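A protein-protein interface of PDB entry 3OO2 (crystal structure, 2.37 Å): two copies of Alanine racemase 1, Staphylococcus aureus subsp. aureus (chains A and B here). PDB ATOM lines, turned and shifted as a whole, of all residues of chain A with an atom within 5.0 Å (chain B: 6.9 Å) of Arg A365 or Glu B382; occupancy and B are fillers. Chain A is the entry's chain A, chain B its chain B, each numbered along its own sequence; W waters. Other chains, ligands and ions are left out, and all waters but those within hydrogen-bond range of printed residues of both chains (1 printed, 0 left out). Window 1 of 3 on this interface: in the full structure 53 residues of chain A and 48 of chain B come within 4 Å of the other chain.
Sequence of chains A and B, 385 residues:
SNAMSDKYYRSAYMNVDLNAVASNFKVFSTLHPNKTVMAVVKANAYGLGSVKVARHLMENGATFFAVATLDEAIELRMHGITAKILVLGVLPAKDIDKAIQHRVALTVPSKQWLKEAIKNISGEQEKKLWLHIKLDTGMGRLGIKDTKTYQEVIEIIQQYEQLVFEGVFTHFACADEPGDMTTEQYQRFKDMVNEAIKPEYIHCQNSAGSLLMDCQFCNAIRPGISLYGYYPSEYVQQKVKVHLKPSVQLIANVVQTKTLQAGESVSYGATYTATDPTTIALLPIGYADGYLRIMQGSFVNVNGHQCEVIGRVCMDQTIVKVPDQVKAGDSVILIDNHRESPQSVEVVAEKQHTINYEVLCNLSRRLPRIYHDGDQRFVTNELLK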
ATOM      1  N   LEU A 363     -29.440  23.023 -15.766  1.00  0.00           N
ATOM      2  CA  LEU A 363     -29.583  21.929 -16.725  1.00  0.00           C
ATOM      3  C   LEU A 363     -28.292  21.768 -17.538  1.00  0.00           C
ATOM      4  O   LEU A 363     -27.961  22.536 -18.418  1.00  0.00           O
ATOM      5  CB  LEU A 363     -30.823  22.162 -17.590  1.00  0.00           C
ATOM      6  CG  LEU A 363     -32.169  21.582 -17.102  1.00  0.00           C
ATOM      7  CD1 LEU A 363     -32.287  21.246 -15.608  1.00  0.00           C
ATOM      8  CD2 LEU A 363     -33.377  22.391 -17.607  1.00  0.00           C
ATOM      9  N   SER A 364     -27.585  20.715 -17.187  1.00  0.00           N
ATOM     10  CA  SER A 364     -26.287  20.327 -17.752  1.00  0.00           C
ATOM     11  C   SER A 364     -26.236  19.893 -19.230  1.00  0.00           C
ATOM     12  O   SER A 364     -27.227  19.508 -19.823  1.00  0.00           O
ATOM     13  CB  SER A 364     -25.741  19.227 -16.833  1.00  0.00           C
ATOM     14  OG  SER A 364     -24.954  18.268 -17.493  1.00  0.00           O
ATOM     15  N   ARG A 365     -25.034  19.910 -19.785  1.00  0.00           N
ATOM     16  CA  ARG A 365     -24.806  19.538 -21.163  1.00  0.00           C
ATOM     17  C   ARG A 365     -25.037  18.080 -21.419  1.00  0.00           C
ATOM     18  O   ARG A 365     -25.106  17.672 -22.579  1.00  0.00           O
ATOM     19  CB  ARG A 365     -23.359  19.813 -21.559  1.00  0.00           C
ATOM     20  CG  ARG A 365     -22.389  18.919 -20.870  1.00  0.00           C
ATOM     21  CD  ARG A 365     -20.939  19.333 -21.102  1.00  0.00           C
ATOM     22  NE  ARG A 365     -20.308  18.897 -22.350  1.00  0.00           N
ATOM     23  CZ  ARG A 365     -19.817  17.673 -22.541  1.00  0.00           C
ATOM     24  NH1 ARG A 365     -19.976  16.740 -21.606  1.00  0.00           N
ATOM     25  NH2 ARG A 365     -19.198  17.359 -23.687  1.00  0.00           N
ATOM     26  N   ARG A 366     -25.080  17.268 -20.368  1.00  0.00           N
ATOM     27  CA  ARG A 366     -25.282  15.848 -20.582  1.00  0.00           C
ATOM     28  C   ARG A 366     -26.730  15.524 -21.000  1.00  0.00           C
ATOM     29  O   ARG A 366     -27.009  14.430 -21.463  1.00  0.00           O
ATOM     30  CB  ARG A 366     -24.831  15.052 -19.367  1.00  0.00           C
ATOM     31  CG  ARG A 366     -24.669  13.575 -19.675  1.00  0.00           C
ATOM     32  CD  ARG A 366     -23.969  12.848 -18.556  1.00  0.00           C
ATOM     33  NE  ARG A 366     -24.764  12.843 -17.316  1.00  0.00           N
ATOM     34  CZ  ARG A 366     -24.413  12.183 -16.224  1.00  0.00           C
ATOM     35  NH1 ARG A 366     -23.285  11.487 -16.209  1.00  0.00           N
ATOM     36  NH2 ARG A 366     -25.180  12.223 -15.143  1.00  0.00           N
ATOM     37  N   LEU A 367     -27.625  16.502 -20.895  1.00  0.00           N
ATOM     38  CA  LEU A 367     -29.018  16.333 -21.272  1.00  0.00           C
ATOM     39  C   LEU A 367     -29.250  16.753 -22.706  1.00  0.00           C
ATOM     40  O   LEU A 367     -28.969  17.871 -23.049  1.00  0.00           O
ATOM     41  CB  LEU A 367     -29.924  17.169 -20.371  1.00  0.00           C
ATOM     42  CG  LEU A 367     -30.085  16.775 -18.903  1.00  0.00           C
ATOM     43  CD1 LEU A 367     -30.684  17.908 -18.102  1.00  0.00           C
ATOM     44  CD2 LEU A 367     -30.924  15.497 -18.753  1.00  0.00           C
ATOM     45  N   ARG A 369     -31.279  18.277 -25.792  1.00  0.00           N
ATOM     46  CA  ARG A 369     -32.437  19.107 -25.941  1.00  0.00           C
ATOM     47  C   ARG A 369     -33.227  18.512 -27.113  1.00  0.00           C
ATOM     48  O   ARG A 369     -32.680  18.306 -28.212  1.00  0.00           O
ATOM     49  CB  ARG A 369     -32.115  20.559 -26.274  1.00  0.00           C
ATOM     50  CG  ARG A 369     -31.077  21.331 -25.466  1.00  0.00           C
ATOM     51  CD  ARG A 369     -30.803  20.842 -24.108  1.00  0.00           C
ATOM     52  NE  ARG A 369     -30.372  21.902 -23.217  1.00  0.00           N
ATOM     53  CZ  ARG A 369     -29.611  21.721 -22.143  1.00  0.00           C
ATOM     54  NH1 ARG A 369     -29.079  20.525 -21.873  1.00  0.00           N
ATOM     55  NH2 ARG A 369     -29.363  22.739 -21.342  1.00  0.00           N
ATOM     56  N   ASN A 381     -27.431  16.813 -28.835  1.00  0.00           N
ATOM     57  CA  ASN A 381     -26.760  16.079 -27.782  1.00  0.00           C
ATOM     58  C   ASN A 381     -25.306  16.507 -27.805  1.00  0.00           C
ATOM     59  O   ASN A 381     -24.513  16.016 -28.609  1.00  0.00           O
ATOM     60  CB  ASN A 381     -26.889  14.569 -28.021  1.00  0.00           C
ATOM     61  CG  ASN A 381     -26.296  13.752 -26.904  1.00  0.00           C
ATOM     62  OD1 ASN A 381     -25.695  14.301 -25.965  1.00  0.00           O
ATOM     63  ND2 ASN A 381     -26.467  12.428 -26.978  1.00  0.00           N
ATOM     64  N   GLU A 382     -24.947  17.411 -26.909  1.00  0.00           N
ATOM     65  CA  GLU A 382     -23.597  17.992 -26.904  1.00  0.00           C
ATOM     66  C   GLU A 382     -22.442  16.988 -26.856  1.00  0.00           C
ATOM     67  O   GLU A 382     -21.397  17.233 -27.434  1.00  0.00           O
ATOM     68  CB  GLU A 382     -23.416  18.937 -25.710  1.00  0.00           C
ATOM     69  CG  GLU A 382     -22.278  19.984 -25.912  1.00  0.00           C
ATOM     70  CD  GLU A 382     -22.799  21.340 -26.414  1.00  0.00           C
ATOM     71  OE1 GLU A 382     -23.862  21.794 -25.897  1.00  0.00           O
ATOM     72  OE2 GLU A 382     -22.130  21.966 -27.282  1.00  0.00           O
ATOM     73  N   LEU A 383     -22.617  15.909 -26.107  1.00  0.00           N
ATOM     74  CA  LEU A 383     -21.610  14.868 -25.986  1.00  0.00           C
ATOM     75  C   LEU A 383     -21.198  14.286 -27.330  1.00  0.00           C
ATOM     76  O   LEU A 383     -20.069  13.830 -27.481  1.00  0.00           O
ATOM     77  CB  LEU A 383     -22.088  13.733 -25.068  1.00  0.00           C
ATOM     78  CG  LEU A 383     -21.955  13.984 -23.558  1.00  0.00           C
ATOM     79  CD1 LEU A 383     -22.780  15.175 -23.097  1.00  0.00           C
ATOM     80  CD2 LEU A 383     -22.324  12.748 -22.707  1.00  0.00           C
ATOM     81  N   ASP B   6      -8.857  25.788 -28.888  1.00  0.00           N
ATOM     82  CA  ASP B   6      -9.908  26.779 -29.114  1.00  0.00           C
ATOM     83  C   ASP B   6      -9.566  28.150 -28.551  1.00  0.00           C
ATOM     84  O   ASP B   6      -8.770  28.272 -27.606  1.00  0.00           O
ATOM     85  CB  ASP B   6     -11.187  26.341 -28.390  1.00  0.00           C
ATOM     86  CG  ASP B   6     -11.855  25.142 -29.013  1.00  0.00           C
ATOM     87  OD1 ASP B   6     -11.913  25.030 -30.261  1.00  0.00           O
ATOM     88  OD2 ASP B   6     -12.404  24.351 -28.234  1.00  0.00           O
ATOM     89  N   ALA B  43     -19.603  11.728 -16.102  1.00  0.00           N
ATOM     90  CA  ALA B  43     -20.054  13.123 -15.983  1.00  0.00           C
ATOM     91  C   ALA B  43     -18.999  14.107 -16.485  1.00  0.00           C
ATOM     92  O   ALA B  43     -18.782  15.146 -15.878  1.00  0.00           O
ATOM     93  CB  ALA B  43     -20.456  13.453 -14.543  1.00  0.00           C
ATOM     94  N   ASN B  44     -18.361  13.769 -17.599  1.00  0.00           N
ATOM     95  CA  ASN B  44     -17.335  14.609 -18.204  1.00  0.00           C
ATOM     96  C   ASN B  44     -16.151  14.737 -17.226  1.00  0.00           C
ATOM     97  O   ASN B  44     -15.642  15.825 -16.962  1.00  0.00           O
ATOM     98  CB  ASN B  44     -17.946  15.961 -18.551  1.00  0.00           C
ATOM     99  CG  ASN B  44     -17.126  16.752 -19.568  1.00  0.00           C
ATOM    100  OD1 ASN B  44     -16.453  16.194 -20.442  1.00  0.00           O
ATOM    101  ND2 ASN B  44     -17.261  18.062 -19.508  1.00  0.00           N
ATOM    102  N   GLY B  49     -13.649  17.581 -18.163  1.00  0.00           N
ATOM    103  CA  GLY B  49     -13.563  17.307 -19.593  1.00  0.00           C
ATOM    104  C   GLY B  49     -12.988  15.897 -19.766  1.00  0.00           C
ATOM    105  O   GLY B  49     -11.774  15.700 -19.729  1.00  0.00           O
ATOM    106  N   SER B  50     -13.874  14.936 -20.005  1.00  0.00           N
ATOM    107  CA  SER B  50     -13.516  13.525 -20.082  1.00  0.00           C
ATOM    108  C   SER B  50     -12.633  13.156 -21.251  1.00  0.00           C
ATOM    109  O   SER B  50     -11.803  12.261 -21.119  1.00  0.00           O
ATOM    110  CB  SER B  50     -14.774  12.663 -20.100  1.00  0.00           C
ATOM    111  OG  SER B  50     -15.541  12.933 -21.244  1.00  0.00           O
ATOM    112  N   VAL B  51     -12.817  13.811 -22.397  1.00  0.00           N
ATOM    113  CA  VAL B  51     -11.978  13.514 -23.565  1.00  0.00           C
ATOM    114  C   VAL B  51     -10.505  13.819 -23.279  1.00  0.00           C
ATOM    115  O   VAL B  51      -9.648  13.000 -23.544  1.00  0.00           O
ATOM    116  CB  VAL B  51     -12.450  14.274 -24.848  1.00  0.00           C
ATOM    117  CG1 VAL B  51     -11.369  14.230 -25.931  1.00  0.00           C
ATOM    118  CG2 VAL B  51     -13.770  13.688 -25.365  1.00  0.00           C
ATOM    119  N   GLU B  72     -21.622   8.828 -23.043  1.00  0.00           N
ATOM    120  CA  GLU B  72     -20.294   9.176 -22.516  1.00  0.00           C
ATOM    121  C   GLU B  72     -19.212   8.284 -23.073  1.00  0.00           C
ATOM    122  O   GLU B  72     -18.135   8.765 -23.395  1.00  0.00           O
ATOM    123  CB  GLU B  72     -20.263   9.156 -20.984  1.00  0.00           C
ATOM    124  CG  GLU B  72     -20.958  10.326 -20.360  1.00  0.00           C
ATOM    125  CD  GLU B  72     -21.032  10.267 -18.861  1.00  0.00           C
ATOM    126  OE1 GLU B  72     -20.813   9.189 -18.289  1.00  0.00           O
ATOM    127  OE2 GLU B  72     -21.332  11.322 -18.251  1.00  0.00           O
ATOM    128  N   GLU B  75     -18.737   9.116 -26.861  1.00  0.00           N
ATOM    129  CA  GLU B  75     -18.045  10.383 -26.965  1.00  0.00           C
ATOM    130  C   GLU B  75     -16.542  10.142 -26.921  1.00  0.00           C
ATOM    131  O   GLU B  75     -15.804  10.713 -27.719  1.00  0.00           O
ATOM    132  CB  GLU B  75     -18.445  11.309 -25.819  1.00  0.00           C
ATOM    133  CG  GLU B  75     -17.799  12.695 -25.887  1.00  0.00           C
ATOM    134  CD  GLU B  75     -18.110  13.568 -24.668  1.00  0.00           C
ATOM    135  OE1 GLU B  75     -18.594  13.032 -23.634  1.00  0.00           O
ATOM    136  OE2 GLU B  75     -17.861  14.792 -24.755  1.00  0.00           O
ATOM    137  N   LEU B 363     -20.322  23.423 -12.732  1.00  0.00           N
ATOM    138  CA  LEU B 363     -19.539  24.221 -13.702  1.00  0.00           C
ATOM    139  C   LEU B 363     -20.035  23.975 -15.164  1.00  0.00           C
ATOM    140  O   LEU B 363     -19.973  22.856 -15.678  1.00  0.00           O
ATOM    141  CB  LEU B 363     -18.056  23.903 -13.496  1.00  0.00           C
ATOM    142  CG  LEU B 363     -17.282  24.713 -12.426  1.00  0.00           C
ATOM    143  CD1 LEU B 363     -18.093  25.551 -11.401  1.00  0.00           C
ATOM    144  CD2 LEU B 363     -16.183  23.892 -11.760  1.00  0.00           C
ATOM    145  N   SER B 364     -20.566  25.030 -15.783  1.00  0.00           N
ATOM    146  CA  SER B 364     -21.238  24.949 -17.089  1.00  0.00           C
ATOM    147  C   SER B 364     -20.357  24.793 -18.274  1.00  0.00           C
ATOM    148  O   SER B 364     -19.199  25.099 -18.226  1.00  0.00           O
ATOM    149  CB  SER B 364     -22.012  26.271 -17.392  1.00  0.00           C
ATOM    150  OG  SER B 364     -23.028  26.518 -16.446  1.00  0.00           O
ATOM    151  N   ARG B 365     -20.989  24.419 -19.381  1.00  0.00           N
ATOM    152  CA  ARG B 365     -20.347  24.363 -20.669  1.00  0.00           C
ATOM    153  C   ARG B 365     -19.832  25.748 -21.063  1.00  0.00           C
ATOM    154  O   ARG B 365     -18.936  25.847 -21.876  1.00  0.00           O
ATOM    155  CB  ARG B 365     -21.342  23.890 -21.735  1.00  0.00           C
ATOM    156  CG  ARG B 365     -22.540  24.805 -21.880  1.00  0.00           C
ATOM    157  CD  ARG B 365     -23.558  24.295 -22.878  1.00  0.00           C
ATOM    158  NE  ARG B 365     -23.104  24.264 -24.265  1.00  0.00           N
ATOM    159  CZ  ARG B 365     -23.165  25.298 -25.115  1.00  0.00           C
ATOM    160  NH1 ARG B 365     -23.632  26.472 -24.735  1.00  0.00           N
ATOM    161  NH2 ARG B 365     -22.763  25.150 -26.371  1.00  0.00           N
ATOM    162  N   ARG B 366     -20.405  26.815 -20.513  1.00  0.00           N
ATOM    163  CA  ARG B 366     -19.975  28.191 -20.879  1.00  0.00           C
ATOM    164  C   ARG B 366     -18.525  28.489 -20.462  1.00  0.00           C
ATOM    165  O   ARG B 366     -17.919  29.398 -20.967  1.00  0.00           O
ATOM    166  CB  ARG B 366     -20.842  29.262 -20.213  1.00  0.00           C
ATOM    167  CG  ARG B 366     -21.184  30.364 -21.167  1.00  0.00           C
ATOM    168  CD  ARG B 366     -21.190  31.788 -20.684  1.00  0.00           C
ATOM    169  NE  ARG B 366     -21.717  32.160 -19.369  1.00  0.00           N
ATOM    170  CZ  ARG B 366     -22.798  32.907 -19.122  1.00  0.00           C
ATOM    171  NH1 ARG B 366     -23.036  33.292 -17.890  1.00  0.00           N
ATOM    172  NH2 ARG B 366     -23.591  33.349 -20.082  1.00  0.00           N
ATOM    173  N   LEU B 367     -18.007  27.785 -19.459  1.00  0.00           N
ATOM    174  CA  LEU B 367     -16.612  27.983 -19.017  1.00  0.00           C
ATOM    175  C   LEU B 367     -15.600  27.243 -19.860  1.00  0.00           C
ATOM    176  O   LEU B 367     -15.715  26.017 -20.034  1.00  0.00           O
ATOM    177  CB  LEU B 367     -16.438  27.471 -17.602  1.00  0.00           C
ATOM    178  CG  LEU B 367     -17.157  28.279 -16.539  1.00  0.00           C
ATOM    179  CD1 LEU B 367     -17.374  27.459 -15.295  1.00  0.00           C
ATOM    180  CD2 LEU B 367     -16.341  29.539 -16.278  1.00  0.00           C
ATOM    181  N   PRO B 368     -14.566  27.963 -20.343  1.00  0.00           N
ATOM    182  CA  PRO B 368     -13.522  27.257 -21.058  1.00  0.00           C
ATOM    183  C   PRO B 368     -12.664  26.496 -20.089  1.00  0.00           C
ATOM    184  O   PRO B 368     -12.477  26.945 -18.978  1.00  0.00           O
ATOM    185  CB  PRO B 368     -12.701  28.383 -21.693  1.00  0.00           C
ATOM    186  CG  PRO B 368     -13.662  29.555 -21.768  1.00  0.00           C
ATOM    187  CD  PRO B 368     -14.410  29.419 -20.475  1.00  0.00           C
ATOM    188  N   ARG B 369     -12.233  25.302 -20.477  1.00  0.00           N
ATOM    189  CA  ARG B 369     -11.328  24.520 -19.686  1.00  0.00           C
ATOM    190  C   ARG B 369      -9.950  24.728 -20.298  1.00  0.00           C
ATOM    191  O   ARG B 369      -9.743  24.462 -21.478  1.00  0.00           O
ATOM    192  CB  ARG B 369     -11.676  23.021 -19.689  1.00  0.00           C
ATOM    193  CG  ARG B 369     -12.717  22.550 -18.680  1.00  0.00           C
ATOM    194  CD  ARG B 369     -14.136  23.025 -18.963  1.00  0.00           C
ATOM    195  NE  ARG B 369     -15.029  22.399 -18.008  1.00  0.00           N
ATOM    196  CZ  ARG B 369     -16.286  22.751 -17.786  1.00  0.00           C
ATOM    197  NH1 ARG B 369     -16.835  23.761 -18.439  1.00  0.00           N
ATOM    198  NH2 ARG B 369     -16.974  22.113 -16.867  1.00  0.00           N
ATOM    199  N   THR B 380     -10.343  24.291 -24.448  1.00  0.00           N
ATOM    200  CA  THR B 380     -11.563  23.654 -24.887  1.00  0.00           C
ATOM    201  C   THR B 380     -12.687  24.659 -24.574  1.00  0.00           C
ATOM    202  O   THR B 380     -12.876  25.030 -23.412  1.00  0.00           O
ATOM    203  CB  THR B 380     -11.778  22.322 -24.150  1.00  0.00           C
ATOM    204  OG1 THR B 380     -10.926  21.314 -24.719  1.00  0.00           O
ATOM    205  CG2 THR B 380     -13.198  21.852 -24.286  1.00  0.00           C
ATOM    206  N   ASN B 381     -13.334  25.193 -25.605  1.00  0.00           N
ATOM    207  CA  ASN B 381     -14.442  26.143 -25.442  1.00  0.00           C
ATOM    208  C   ASN B 381     -15.572  25.479 -26.184  1.00  0.00           C
ATOM    209  O   ASN B 381     -15.639  25.540 -27.396  1.00  0.00           O
ATOM    210  CB  ASN B 381     -14.102  27.511 -26.040  1.00  0.00           C
ATOM    211  CG  ASN B 381     -15.177  28.574 -25.764  1.00  0.00           C
ATOM    212  OD1 ASN B 381     -16.195  28.298 -25.150  1.00  0.00           O
ATOM    213  ND2 ASN B 381     -14.929  29.801 -26.215  1.00  0.00           N
ATOM    214  N   GLU B 382     -16.437  24.779 -25.449  1.00  0.00           N
ATOM    215  CA  GLU B 382     -17.524  24.010 -26.066  1.00  0.00           C
ATOM    216  C   GLU B 382     -18.445  24.854 -26.980  1.00  0.00           C
ATOM    217  O   GLU B 382     -18.966  24.343 -27.972  1.00  0.00           O
ATOM    218  CB  GLU B 382     -18.298  23.255 -24.981  1.00  0.00           C
ATOM    219  CG  GLU B 382     -18.802  21.898 -25.453  1.00  0.00           C
ATOM    220  CD  GLU B 382     -18.788  20.820 -24.345  1.00  0.00           C
ATOM    221  OE1 GLU B 382     -19.355  21.045 -23.251  1.00  0.00           O
ATOM    222  OE2 GLU B 382     -18.244  19.718 -24.602  1.00  0.00           O
ATOM    223  N   LEU B 383     -18.562  26.149 -26.698  1.00  0.00           N
ATOM    224  CA  LEU B 383     -19.376  27.043 -27.510  1.00  0.00           C
ATOM    225  C   LEU B 383     -18.863  27.273 -28.945  1.00  0.00           C
ATOM    226  O   LEU B 383     -19.657  27.615 -29.826  1.00  0.00           O
ATOM    227  CB  LEU B 383     -19.580  28.405 -26.831  1.00  0.00           C
ATOM    228  CG  LEU B 383     -20.705  28.580 -25.831  1.00  0.00           C
ATOM    229  CD1 LEU B 383     -20.574  27.701 -24.564  1.00  0.00           C
ATOM    230  CD2 LEU B 383     -20.800  30.049 -25.461  1.00  0.00           C
ATOM    231  N   LEU B 384     -17.547  27.159 -29.149  1.00  0.00           N
ATOM    232  CA  LEU B 384     -16.927  27.348 -30.463  1.00  0.00           C
ATOM    233  C   LEU B 384     -16.430  26.024 -31.009  1.00  0.00           C
ATOM    234  O   LEU B 384     -15.758  25.957 -32.047  1.00  0.00           O
ATOM    235  CB  LEU B 384     -15.725  28.270 -30.344  1.00  0.00           C
ATOM    236  CG  LEU B 384     -15.942  29.607 -29.644  1.00  0.00           C
ATOM    237  CD1 LEU B 384     -14.620  30.380 -29.696  1.00  0.00           C
ATOM    238  CD2 LEU B 384     -17.089  30.411 -30.272  1.00  0.00           C
ATOM    239  N   LYS B 385     -16.770  24.970 -30.290  1.00  0.00           N
ATOM    240  CA  LYS B 385     -16.346  23.629 -30.579  1.00  0.00           C
ATOM    241  C   LYS B 385     -17.426  22.990 -31.399  1.00  0.00           C
ATOM    242  O   LYS B 385     -17.750  23.478 -32.488  1.00  0.00           O
ATOM    243  CB  LYS B 385     -16.186  22.901 -29.242  1.00  0.00           C
ATOM    244  CG  LYS B 385     -15.598  21.495 -29.259  1.00  0.00           C
ATOM    245  CD  LYS B 385     -15.456  20.998 -27.780  1.00  0.00           C
ATOM    246  CE  LYS B 385     -14.852  19.603 -27.652  1.00  0.00           C
ATOM    247  NZ  LYS B 385     -14.784  19.162 -26.206  1.00  0.00           N
ATOM    248  OXT LYS B 385     -17.986  21.976 -30.958  1.00  0.00           O
HETATM  249  O   HOH W   1     -18.557  14.134 -21.344  1.00  0.00           O
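OE2 of Glu B75 is in salt-bridge range of NH2 of Arg A365, 3.1 Å away. The guanidinium group (NE) of Arg A365 lies within salt-bridge range of the side-chain carboxylate (OE1) of Glu B382, 2.5 Å away. The guanidinium group (NH1) of Arg A366 is in salt-bridge range of the side-chain carboxylate (OE2) of Glu B72, at 2.8 Å. NE of Arg B365 lies within salt-bridge range of OE1 of Glu A382 (3.1 Å).
The backbone NH (N) of Arg A366 sits at hydrogen-bond distance from the side-chain hydroxyl (OG) of Ser A364 (3.0 Å). The side-chain amide oxygen (OD1) of Asn A381 lies close to the backbone NH (N) of Leu A383 (3.5 Å). OE2 of Glu B72 sits at hydrogen-bond distance from N of Ala B43 (2.8 Å). The backbone carbonyl oxygen of Asn B44 is in hydrogen-bond range of the backbone NH of Gly B49, 2.9 Å away. OD1 of Asn B44 lies within hydrogen-bond range of N of Ser B50 (2.9 Å). The side-chain carboxylate (OE2) of Glu B382 lies within salt-bridge range of the side-chain amino group (NZ) of Lys B385 (3.9 Å).
Arg A365 touches Asn B44 (NH1 to CG, 3.5 Å). NH1 of Arg A366 touches CA of Ala B43, at 3.6 Å. OE2 of Glu A382 touches CG of Glu B382, 3.8 Å away. Leu A383 touches Glu B72 (CD2 to CG, 3.6 Å). Glu B75 touches Leu A383 (CG to O, 3.0 Å).
Of chain B, only Asn B44 (3.5 Å), Glu B75 (3.1 Å) and Glu B382 (2.5 Å) come within 4 Å of Arg A365. Printed residues of chain B within 4 Å of Arg A366: Ala B43 and Glu B72. Gly B49 touches none of the printed residues of chain A. Of the printed residues of chain A, Glu B72 touches Arg A366 (2.8 Å) and Leu A383 (3.6 Å). Of the printed residues of chain A, Glu B75 touches Arg A365 (3.1 Å) and Leu A383 (3.0 Å). Of the printed residues of chain A, Arg B365 touches Glu A382. Of chain A, only Arg A365 (2.5 Å) and Glu A382 (3.8 Å) come within 4 Å of Glu B382. The nearest residue of chain B that does not touch Arg A365 is Arg B365 (4.6 Å).
Printed residues of chain B that touch a printed residue of chain A: Ala B43, Asn B44, Glu B72, Glu B75, Arg B365 and Glu B382. Hydrophobic or aromatic side chains of chain B that line the printed part of chain A: Ala B43. Along chain B the printed residues that touch a printed residue of chain A span positions 43 to 382. Printed residues of chain A that touch a printed residue of chain B: Arg A365, Arg A366, Glu A382 and Leu A383. Hydrophobic or aromatic side chains of chain A within 4 Å of the printed part of chain B: Leu A383. Among the printed residues, Asp or Glu carboxylates within 4 Å of a Lys or Arg side-chain nitrogen of the other chain: Arg A365 with Glu B75 (3.1 Å), Arg A365 with Glu B382 (2.5 Å), Arg A366 with Glu B72 (2.8 Å) and Glu A382 with Arg B365 (3.1 Å).
Arg A365 touches Glu B382, and with the chains exchanged Glu A382 touches Arg B365. Glu B382 touches its own counterpart, Glu A382.
Water W1 lies within hydrogen-bond range of the side-chain carboxylate (OE1) of Glu B75 (2.5 Å), the guanidinium group (NH1) of Arg A365 (3.0 Å), the side-chain amide oxygen (OD1) of Asn B44 (3.1 Å) and the side-chain hydroxyl (OG) of Ser B50 (3.2 Å).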
